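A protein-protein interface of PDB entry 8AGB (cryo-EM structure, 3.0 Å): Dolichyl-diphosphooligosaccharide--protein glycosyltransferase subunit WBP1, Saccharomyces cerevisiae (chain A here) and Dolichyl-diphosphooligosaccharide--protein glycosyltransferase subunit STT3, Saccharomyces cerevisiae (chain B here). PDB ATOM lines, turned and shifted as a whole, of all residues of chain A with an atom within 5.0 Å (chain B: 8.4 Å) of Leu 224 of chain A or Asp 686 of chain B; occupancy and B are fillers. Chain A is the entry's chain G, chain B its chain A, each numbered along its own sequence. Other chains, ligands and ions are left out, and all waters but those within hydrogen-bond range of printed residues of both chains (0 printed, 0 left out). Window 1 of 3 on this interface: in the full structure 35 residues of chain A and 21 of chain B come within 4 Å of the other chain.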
ATOM      1  N   GLU A 104      20.516  15.146 -30.706  1.00  0.00           N
ATOM      2  CA  GLU A 104      19.079  15.404 -30.599  1.00  0.00           C
ATOM      3  C   GLU A 104      18.259  14.203 -31.056  1.00  0.00           C
ATOM      4  O   GLU A 104      17.297  13.803 -30.393  1.00  0.00           O
ATOM      5  CB  GLU A 104      18.705  16.647 -31.406  1.00  0.00           C
ATOM      6  CG  GLU A 104      19.331  17.929 -30.895  1.00  0.00           C
ATOM      7  CD  GLU A 104      18.533  19.154 -31.279  1.00  0.00           C
ATOM      8  OE1 GLU A 104      17.311  19.021 -31.494  1.00  0.00           O
ATOM      9  OE2 GLU A 104      19.127  20.247 -31.370  1.00  0.00           O
ATOM     10  N   GLN A 187      19.501  17.685 -16.555  1.00  0.00           N
ATOM     11  CA  GLN A 187      19.948  16.617 -17.436  1.00  0.00           C
ATOM     12  C   GLN A 187      21.314  16.074 -17.056  1.00  0.00           C
ATOM     13  O   GLN A 187      21.571  14.881 -17.247  1.00  0.00           O
ATOM     14  CB  GLN A 187      19.993  17.117 -18.880  1.00  0.00           C
ATOM     15  CG  GLN A 187      18.641  17.197 -19.547  1.00  0.00           C
ATOM     16  CD  GLN A 187      18.072  18.595 -19.498  1.00  0.00           C
ATOM     17  OE1 GLN A 187      18.809  19.570 -19.390  1.00  0.00           O
ATOM     18  NE2 GLN A 187      16.754  18.701 -19.565  1.00  0.00           N
ATOM     19  N   GLN A 222      22.049  12.997 -19.976  1.00  0.00           N
ATOM     20  CA  GLN A 222      20.933  12.290 -20.588  1.00  0.00           C
ATOM     21  C   GLN A 222      20.019  13.302 -21.260  1.00  0.00           C
ATOM     22  O   GLN A 222      19.406  14.139 -20.591  1.00  0.00           O
ATOM     23  CB  GLN A 222      20.167  11.474 -19.554  1.00  0.00           C
ATOM     24  CG  GLN A 222      19.084  10.606 -20.158  1.00  0.00           C
ATOM     25  CD  GLN A 222      18.261   9.898 -19.112  1.00  0.00           C
ATOM     26  OE1 GLN A 222      17.037   9.992 -19.104  1.00  0.00           O
ATOM     27  NE2 GLN A 222      18.928   9.183 -18.220  1.00  0.00           N
ATOM     28  N   ASN A 223      19.940  13.220 -22.583  1.00  0.00           N
ATOM     29  CA  ASN A 223      19.117  14.108 -23.382  1.00  0.00           C
ATOM     30  C   ASN A 223      17.648  13.992 -22.971  1.00  0.00           C
ATOM     31  O   ASN A 223      17.244  13.076 -22.253  1.00  0.00           O
ATOM     32  CB  ASN A 223      19.289  13.766 -24.859  1.00  0.00           C
ATOM     33  CG  ASN A 223      18.906  14.896 -25.757  1.00  0.00           C
ATOM     34  OD1 ASN A 223      18.565  15.973 -25.286  1.00  0.00           O
ATOM     35  ND2 ASN A 223      18.956  14.665 -27.062  1.00  0.00           N
ATOM     36  N   LEU A 224      16.834  14.939 -23.440  1.00  0.00           N
ATOM     37  CA  LEU A 224      15.401  14.838 -23.193  1.00  0.00           C
ATOM     38  C   LEU A 224      14.741  13.751 -24.029  1.00  0.00           C
ATOM     39  O   LEU A 224      13.575  13.425 -23.784  1.00  0.00           O
ATOM     40  CB  LEU A 224      14.715  16.176 -23.457  1.00  0.00           C
ATOM     41  CG  LEU A 224      14.943  17.252 -22.400  1.00  0.00           C
ATOM     42  CD1 LEU A 224      14.056  18.450 -22.670  1.00  0.00           C
ATOM     43  CD2 LEU A 224      14.662  16.679 -21.026  1.00  0.00           C
ATOM     44  N   ASN A 225      15.452  13.193 -25.005  1.00  0.00           N
ATOM     45  CA  ASN A 225      14.990  12.050 -25.778  1.00  0.00           C
ATOM     46  C   ASN A 225      15.591  10.742 -25.290  1.00  0.00           C
ATOM     47  O   ASN A 225      15.537   9.741 -26.010  1.00  0.00           O
ATOM     48  CB  ASN A 225      15.299  12.260 -27.259  1.00  0.00           C
ATOM     49  CG  ASN A 225      14.809  13.599 -27.764  1.00  0.00           C
ATOM     50  OD1 ASN A 225      15.558  14.359 -28.374  1.00  0.00           O
ATOM     51  ND2 ASN A 225      13.540  13.894 -27.514  1.00  0.00           N
ATOM     52  N   ASN A 226      16.193  10.746 -24.099  1.00  0.00           N
ATOM     53  CA  ASN A 226      16.823   9.576 -23.495  1.00  0.00           C
ATOM     54  C   ASN A 226      18.087   9.150 -24.237  1.00  0.00           C
ATOM     55  O   ASN A 226      18.435   7.970 -24.253  1.00  0.00           O
ATOM     56  CB  ASN A 226      15.845   8.403 -23.375  1.00  0.00           C
ATOM     57  CG  ASN A 226      14.715   8.689 -22.406  1.00  0.00           C
ATOM     58  OD1 ASN A 226      13.588   8.240 -22.599  1.00  0.00           O
ATOM     59  ND2 ASN A 226      15.013   9.444 -21.360  1.00  0.00           N
ATOM     60  N   ARG A 360      11.248  11.089 -13.020  1.00  0.00           N
ATOM     61  CA  ARG A 360      12.514  11.705 -13.413  1.00  0.00           C
ATOM     62  C   ARG A 360      13.501  11.513 -12.268  1.00  0.00           C
ATOM     63  O   ARG A 360      13.625  12.372 -11.392  1.00  0.00           O
ATOM     64  CB  ARG A 360      12.336  13.180 -13.753  1.00  0.00           C
ATOM     65  CG  ARG A 360      11.181  13.478 -14.683  1.00  0.00           C
ATOM     66  CD  ARG A 360      10.883  14.963 -14.711  1.00  0.00           C
ATOM     67  NE  ARG A 360      11.659  15.663 -15.729  1.00  0.00           N
ATOM     68  CZ  ARG A 360      11.396  15.622 -17.030  1.00  0.00           C
ATOM     69  NH1 ARG A 360      10.371  14.912 -17.481  1.00  0.00           N
ATOM     70  NH2 ARG A 360      12.155  16.294 -17.884  1.00  0.00           N
ATOM     71  N   TYR B 558       6.719  33.108 -23.374  1.00  0.00           N
ATOM     72  CA  TYR B 558       6.842  31.664 -23.530  1.00  0.00           C
ATOM     73  C   TYR B 558       6.468  30.941 -22.245  1.00  0.00           C
ATOM     74  O   TYR B 558       5.716  29.962 -22.270  1.00  0.00           O
ATOM     75  CB  TYR B 558       8.265  31.303 -23.954  1.00  0.00           C
ATOM     76  CG  TYR B 558       8.465  29.836 -24.246  1.00  0.00           C
ATOM     77  CD1 TYR B 558       7.985  29.271 -25.417  1.00  0.00           C
ATOM     78  CD2 TYR B 558       9.136  29.017 -23.353  1.00  0.00           C
ATOM     79  CE1 TYR B 558       8.167  27.936 -25.689  1.00  0.00           C
ATOM     80  CE2 TYR B 558       9.322  27.679 -23.617  1.00  0.00           C
ATOM     81  CZ  TYR B 558       8.836  27.144 -24.785  1.00  0.00           C
ATOM     82  OH  TYR B 558       9.020  25.809 -25.051  1.00  0.00           O
ATOM     83  N   TYR B 665      11.602  32.084 -29.710  1.00  0.00           N
ATOM     84  CA  TYR B 665      10.781  31.074 -29.059  1.00  0.00           C
ATOM     85  C   TYR B 665       9.575  30.632 -29.872  1.00  0.00           C
ATOM     86  O   TYR B 665       8.977  29.605 -29.539  1.00  0.00           O
ATOM     87  CB  TYR B 665      10.293  31.577 -27.692  1.00  0.00           C
ATOM     88  CG  TYR B 665      11.392  31.797 -26.679  1.00  0.00           C
ATOM     89  CD1 TYR B 665      12.247  32.885 -26.775  1.00  0.00           C
ATOM     90  CD2 TYR B 665      11.570  30.921 -25.622  1.00  0.00           C
ATOM     91  CE1 TYR B 665      13.247  33.087 -25.850  1.00  0.00           C
ATOM     92  CE2 TYR B 665      12.566  31.114 -24.695  1.00  0.00           C
ATOM     93  CZ  TYR B 665      13.401  32.198 -24.813  1.00  0.00           C
ATOM     94  OH  TYR B 665      14.397  32.395 -23.889  1.00  0.00           O
ATOM     95  N   LYS B 683       7.571  26.637 -29.999  1.00  0.00           N
ATOM     96  CA  LYS B 683       8.504  25.558 -30.276  1.00  0.00           C
ATOM     97  C   LYS B 683       8.849  24.818 -28.992  1.00  0.00           C
ATOM     98  O   LYS B 683       8.891  25.400 -27.905  1.00  0.00           O
ATOM     99  CB  LYS B 683       9.785  26.077 -30.929  1.00  0.00           C
ATOM    100  CG  LYS B 683      10.625  26.972 -30.047  1.00  0.00           C
ATOM    101  CD  LYS B 683      11.455  27.950 -30.862  1.00  0.00           C
ATOM    102  CE  LYS B 683      11.923  27.339 -32.166  1.00  0.00           C
ATOM    103  NZ  LYS B 683      12.565  28.350 -33.045  1.00  0.00           N
ATOM    104  N   LYS B 684       9.080  23.517 -29.124  1.00  0.00           N
ATOM    105  CA  LYS B 684       9.318  22.680 -27.960  1.00  0.00           C
ATOM    106  C   LYS B 684      10.679  22.998 -27.359  1.00  0.00           C
ATOM    107  O   LYS B 684      11.632  23.315 -28.076  1.00  0.00           O
ATOM    108  CB  LYS B 684       9.240  21.205 -28.345  1.00  0.00           C
ATOM    109  CG  LYS B 684       9.949  20.874 -29.643  1.00  0.00           C
ATOM    110  CD  LYS B 684       9.387  19.610 -30.268  1.00  0.00           C
ATOM    111  CE  LYS B 684       9.567  18.413 -29.353  1.00  0.00           C
ATOM    112  NZ  LYS B 684       8.883  17.203 -29.885  1.00  0.00           N
ATOM    113  N   ASP B 685      10.758  22.928 -26.031  1.00  0.00           N
ATOM    114  CA  ASP B 685      11.986  23.266 -25.325  1.00  0.00           C
ATOM    115  C   ASP B 685      13.148  22.430 -25.842  1.00  0.00           C
ATOM    116  O   ASP B 685      12.971  21.299 -26.304  1.00  0.00           O
ATOM    117  CB  ASP B 685      11.811  23.049 -23.825  1.00  0.00           C
ATOM    118  CG  ASP B 685      10.954  21.844 -23.511  1.00  0.00           C
ATOM    119  OD1 ASP B 685      10.563  21.134 -24.461  1.00  0.00           O
ATOM    120  OD2 ASP B 685      10.668  21.607 -22.319  1.00  0.00           O
ATOM    121  N   ASP B 686      14.348  22.999 -25.760  1.00  0.00           N
ATOM    122  CA  ASP B 686      15.514  22.343 -26.332  1.00  0.00           C
ATOM    123  C   ASP B 686      15.796  21.029 -25.619  1.00  0.00           C
ATOM    124  O   ASP B 686      15.635  20.911 -24.403  1.00  0.00           O
ATOM    125  CB  ASP B 686      16.738  23.252 -26.263  1.00  0.00           C
ATOM    126  CG  ASP B 686      17.821  22.822 -27.228  1.00  0.00           C
ATOM    127  OD1 ASP B 686      17.548  21.934 -28.060  1.00  0.00           O
ATOM    128  OD2 ASP B 686      18.939  23.365 -27.167  1.00  0.00           O
ATOM    129  N   ALA B 687      16.222  20.036 -26.400  1.00  0.00           N
ATOM    130  CA  ALA B 687      16.521  18.723 -25.846  1.00  0.00           C
ATOM    131  C   ALA B 687      17.710  18.781 -24.895  1.00  0.00           C
ATOM    132  O   ALA B 687      17.667  18.216 -23.798  1.00  0.00           O
ATOM    133  CB  ALA B 687      16.770  17.733 -26.981  1.00  0.00           C
ATOM    134  N   GLN B 688      18.783  19.464 -25.292  1.00  0.00           N
ATOM    135  CA  GLN B 688      19.937  19.606 -24.412  1.00  0.00           C
ATOM    136  C   GLN B 688      19.667  20.507 -23.214  1.00  0.00           C
ATOM    137  O   GLN B 688      20.596  20.774 -22.445  1.00  0.00           O
ATOM    138  CB  GLN B 688      21.140  20.135 -25.195  1.00  0.00           C
ATOM    139  CG  GLN B 688      21.718  19.154 -26.202  1.00  0.00           C
ATOM    140  CD  GLN B 688      20.826  18.941 -27.403  1.00  0.00           C
ATOM    141  OE1 GLN B 688      20.121  19.850 -27.837  1.00  0.00           O
ATOM    142  NE2 GLN B 688      20.844  17.732 -27.944  1.00  0.00           N
ATOM    143  N   GLY B 689      18.438  20.982 -23.040  1.00  0.00           N
ATOM    144  CA  GLY B 689      18.058  21.768 -21.885  1.00  0.00           C
ATOM    145  C   GLY B 689      18.784  23.085 -21.722  1.00  0.00           C
ATOM    146  O   GLY B 689      19.241  23.413 -20.624  1.00  0.00           O
ATOM    147  N   ARG B 690      18.894  23.853 -22.800  1.00  0.00           N
ATOM    148  CA  ARG B 690      19.422  25.205 -22.739  1.00  0.00           C
ATOM    149  C   ARG B 690      18.343  26.184 -23.178  1.00  0.00           C
ATOM    150  O   ARG B 690      17.348  25.806 -23.802  1.00  0.00           O
ATOM    151  CB  ARG B 690      20.670  25.366 -23.613  1.00  0.00           C
ATOM    152  CG  ARG B 690      20.473  24.929 -25.036  1.00  0.00           C
ATOM    153  CD  ARG B 690      21.688  24.207 -25.574  1.00  0.00           C
ATOM    154  NE  ARG B 690      21.415  23.613 -26.877  1.00  0.00           N
ATOM    155  CZ  ARG B 690      22.054  23.937 -27.994  1.00  0.00           C
ATOM    156  NH1 ARG B 690      23.012  24.852 -27.969  1.00  0.00           N
ATOM    157  NH2 ARG B 690      21.736  23.346 -29.137  1.00  0.00           N
ATOM    158  N   THR B 691      18.607  27.461 -22.918  1.00  0.00           N
ATOM    159  CA  THR B 691      17.631  28.516 -23.237  1.00  0.00           C
ATOM    160  C   THR B 691      17.494  28.603 -24.736  1.00  0.00           C
ATOM    161  O   THR B 691      18.509  28.565 -25.408  1.00  0.00           O
ATOM    162  CB  THR B 691      18.173  29.854 -22.756  1.00  0.00           C
ATOM    163  OG1 THR B 691      19.371  29.544 -22.054  1.00  0.00           O
ATOM    164  CG2 THR B 691      17.219  30.574 -21.831  1.00  0.00           C
ATOM    165  N   LEU B 692      16.272  28.702 -25.219  1.00  0.00           N
ATOM    166  CA  LEU B 692      16.077  28.863 -26.656  1.00  0.00           C
ATOM    167  C   LEU B 692      16.746  30.125 -27.180  1.00  0.00           C
ATOM    168  O   LEU B 692      17.116  30.187 -28.359  1.00  0.00           O
ATOM    169  CB  LEU B 692      14.585  28.870 -26.982  1.00  0.00           C
ATOM    170  CG  LEU B 692      13.870  27.530 -26.808  1.00  0.00           C
ATOM    171  CD1 LEU B 692      12.368  27.713 -26.827  1.00  0.00           C
ATOM    172  CD2 LEU B 692      14.306  26.559 -27.887  1.00  0.00           C
ATOM    173  N   ARG B 693      16.914  31.139 -26.329  1.00  0.00           N
ATOM    174  CA  ARG B 693      17.596  32.351 -26.766  1.00  0.00           C
ATOM    175  C   ARG B 693      19.057  32.074 -27.097  1.00  0.00           C
ATOM    176  O   ARG B 693      19.594  32.628 -28.061  1.00  0.00           O
ATOM    177  CB  ARG B 693      17.489  33.429 -25.692  1.00  0.00           C
ATOM    178  CG  ARG B 693      18.459  34.572 -25.889  1.00  0.00           C
ATOM    179  CD  ARG B 693      18.478  35.503 -24.698  1.00  0.00           C
ATOM    180  NE  ARG B 693      19.528  36.507 -24.826  1.00  0.00           N
ATOM    181  CZ  ARG B 693      20.679  36.468 -24.165  1.00  0.00           C
ATOM    182  NH1 ARG B 693      21.582  37.422 -24.343  1.00  0.00           N
ATOM    183  NH2 ARG B 693      20.928  35.475 -23.323  1.00  0.00           N
ATOM    184  N   ASP B 694      19.712  31.205 -26.325  1.00  0.00           N
ATOM    185  CA  ASP B 694      21.103  30.874 -26.616  1.00  0.00           C
ATOM    186  C   ASP B 694      21.215  30.050 -27.891  1.00  0.00           C
ATOM    187  O   ASP B 694      22.135  30.256 -28.689  1.00  0.00           O
ATOM    188  CB  ASP B 694      21.734  30.140 -25.435  1.00  0.00           C
ATOM    189  CG  ASP B 694      21.981  31.050 -24.250  1.00  0.00           C
ATOM    190  OD1 ASP B 694      21.078  31.189 -23.402  1.00  0.00           O
ATOM    191  OD2 ASP B 694      23.083  31.631 -24.167  1.00  0.00           O
ATOM    192  N   VAL B 695      20.289  29.112 -28.098  1.00  0.00           N
ATOM    193  CA  VAL B 695      20.226  28.385 -29.363  1.00  0.00           C
ATOM    194  C   VAL B 695      20.117  29.361 -30.526  1.00  0.00           C
ATOM    195  O   VAL B 695      20.852  29.265 -31.517  1.00  0.00           O
ATOM    196  CB  VAL B 695      19.050  27.393 -29.352  1.00  0.00           C
ATOM    197  CG1 VAL B 695      19.033  26.582 -30.633  1.00  0.00           C
ATOM    198  CG2 VAL B 695      19.132  26.489 -28.141  1.00  0.00           C
ATOM    199  N   GLY B 696      19.175  30.298 -30.431  1.00  0.00           N
ATOM    200  CA  GLY B 696      19.001  31.309 -31.453  1.00  0.00           C
ATOM    201  C   GLY B 696      20.265  32.097 -31.719  1.00  0.00           C
ATOM    202  O   GLY B 696      20.704  32.181 -32.865  1.00  0.00           O
ATOM    203  N   LEU B 698      23.220  31.345 -31.142  1.00  0.00           N
ATOM    204  CA  LEU B 698      24.249  30.486 -31.718  1.00  0.00           C
ATOM    205  C   LEU B 698      24.049  30.300 -33.216  1.00  0.00           C
ATOM    206  O   LEU B 698      24.995  30.440 -33.999  1.00  0.00           O
ATOM    207  CB  LEU B 698      24.254  29.135 -31.005  1.00  0.00           C
ATOM    208  CG  LEU B 698      25.102  28.041 -31.653  1.00  0.00           C
ATOM    209  CD1 LEU B 698      26.573  28.269 -31.359  1.00  0.00           C
ATOM    210  CD2 LEU B 698      24.660  26.671 -31.173  1.00  0.00           C
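Printed residues of chain B within 4 Å of Gln 187 of chain A: Gln 688 (3.7 Å) and Gly 689 (3.4 Å). Asn 223 of chain A touches two residues of chain B. Leu 224 of chain A touches just these residues of chain B: Asp 686 and Ala 687. Of the printed residues of chain B, Asn 225 of chain A touches Ala 687 (3.8 Å). Of the printed residues of chain A, Asp 686 of chain B touches Leu 224 (3.4 Å). Of the printed residues of chain A, Ala 687 of chain B touches Asn 223, Leu 224 and Asn 225. The nearest residue of chain B that does not touch Leu 224 of chain A is Asp 685 of chain B (4.6 Å).
Glu 104 of chain A touches Gln 688 of chain B. Gln 187 of chain A touches Gln 688 of chain B. Gly 689 of chain B touches Gln 187 of chain A (CA to OE1, 3.4 Å). Asp 686 of chain B touches Leu 224 of chain A (O to CD1, 3.4 Å). Asn 225 of chain A touches Ala 687 of chain B.
The backbone carbonyl oxygen of Ala 687 of chain B lies close to the side-chain amide oxygen of Asn 223 of chain A (2.8 Å). The backbone carbonyl oxygen (O) of Ala 687 of chain B sits close to the backbone NH (N) of Leu 224 of chain A. The backbone NH of Gln 688 of chain B lies within hydrogen-bond range of the side-chain amide oxygen of Asn 223 of chain A (3.5 Å).
The side-chain carboxylate (OD1) of Asp 686 of chain B sits close to the side-chain amide oxygen (OE1) of Gln 688 of chain B, 3.3 Å away. The guanidinium group of Arg 690 of chain B is in salt-bridge range of the side-chain carboxylate of Asp 686 of chain B, at 2.5 Å. O of Glu 104 of chain A sits close to OD1 of Asn 225 of chain A. N of Gln 222 of chain A sits at hydrogen-bond distance from O of Gln 187 of chain A.
Along chain A the printed residues that touch a printed residue of chain B span positions 104 to 225.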
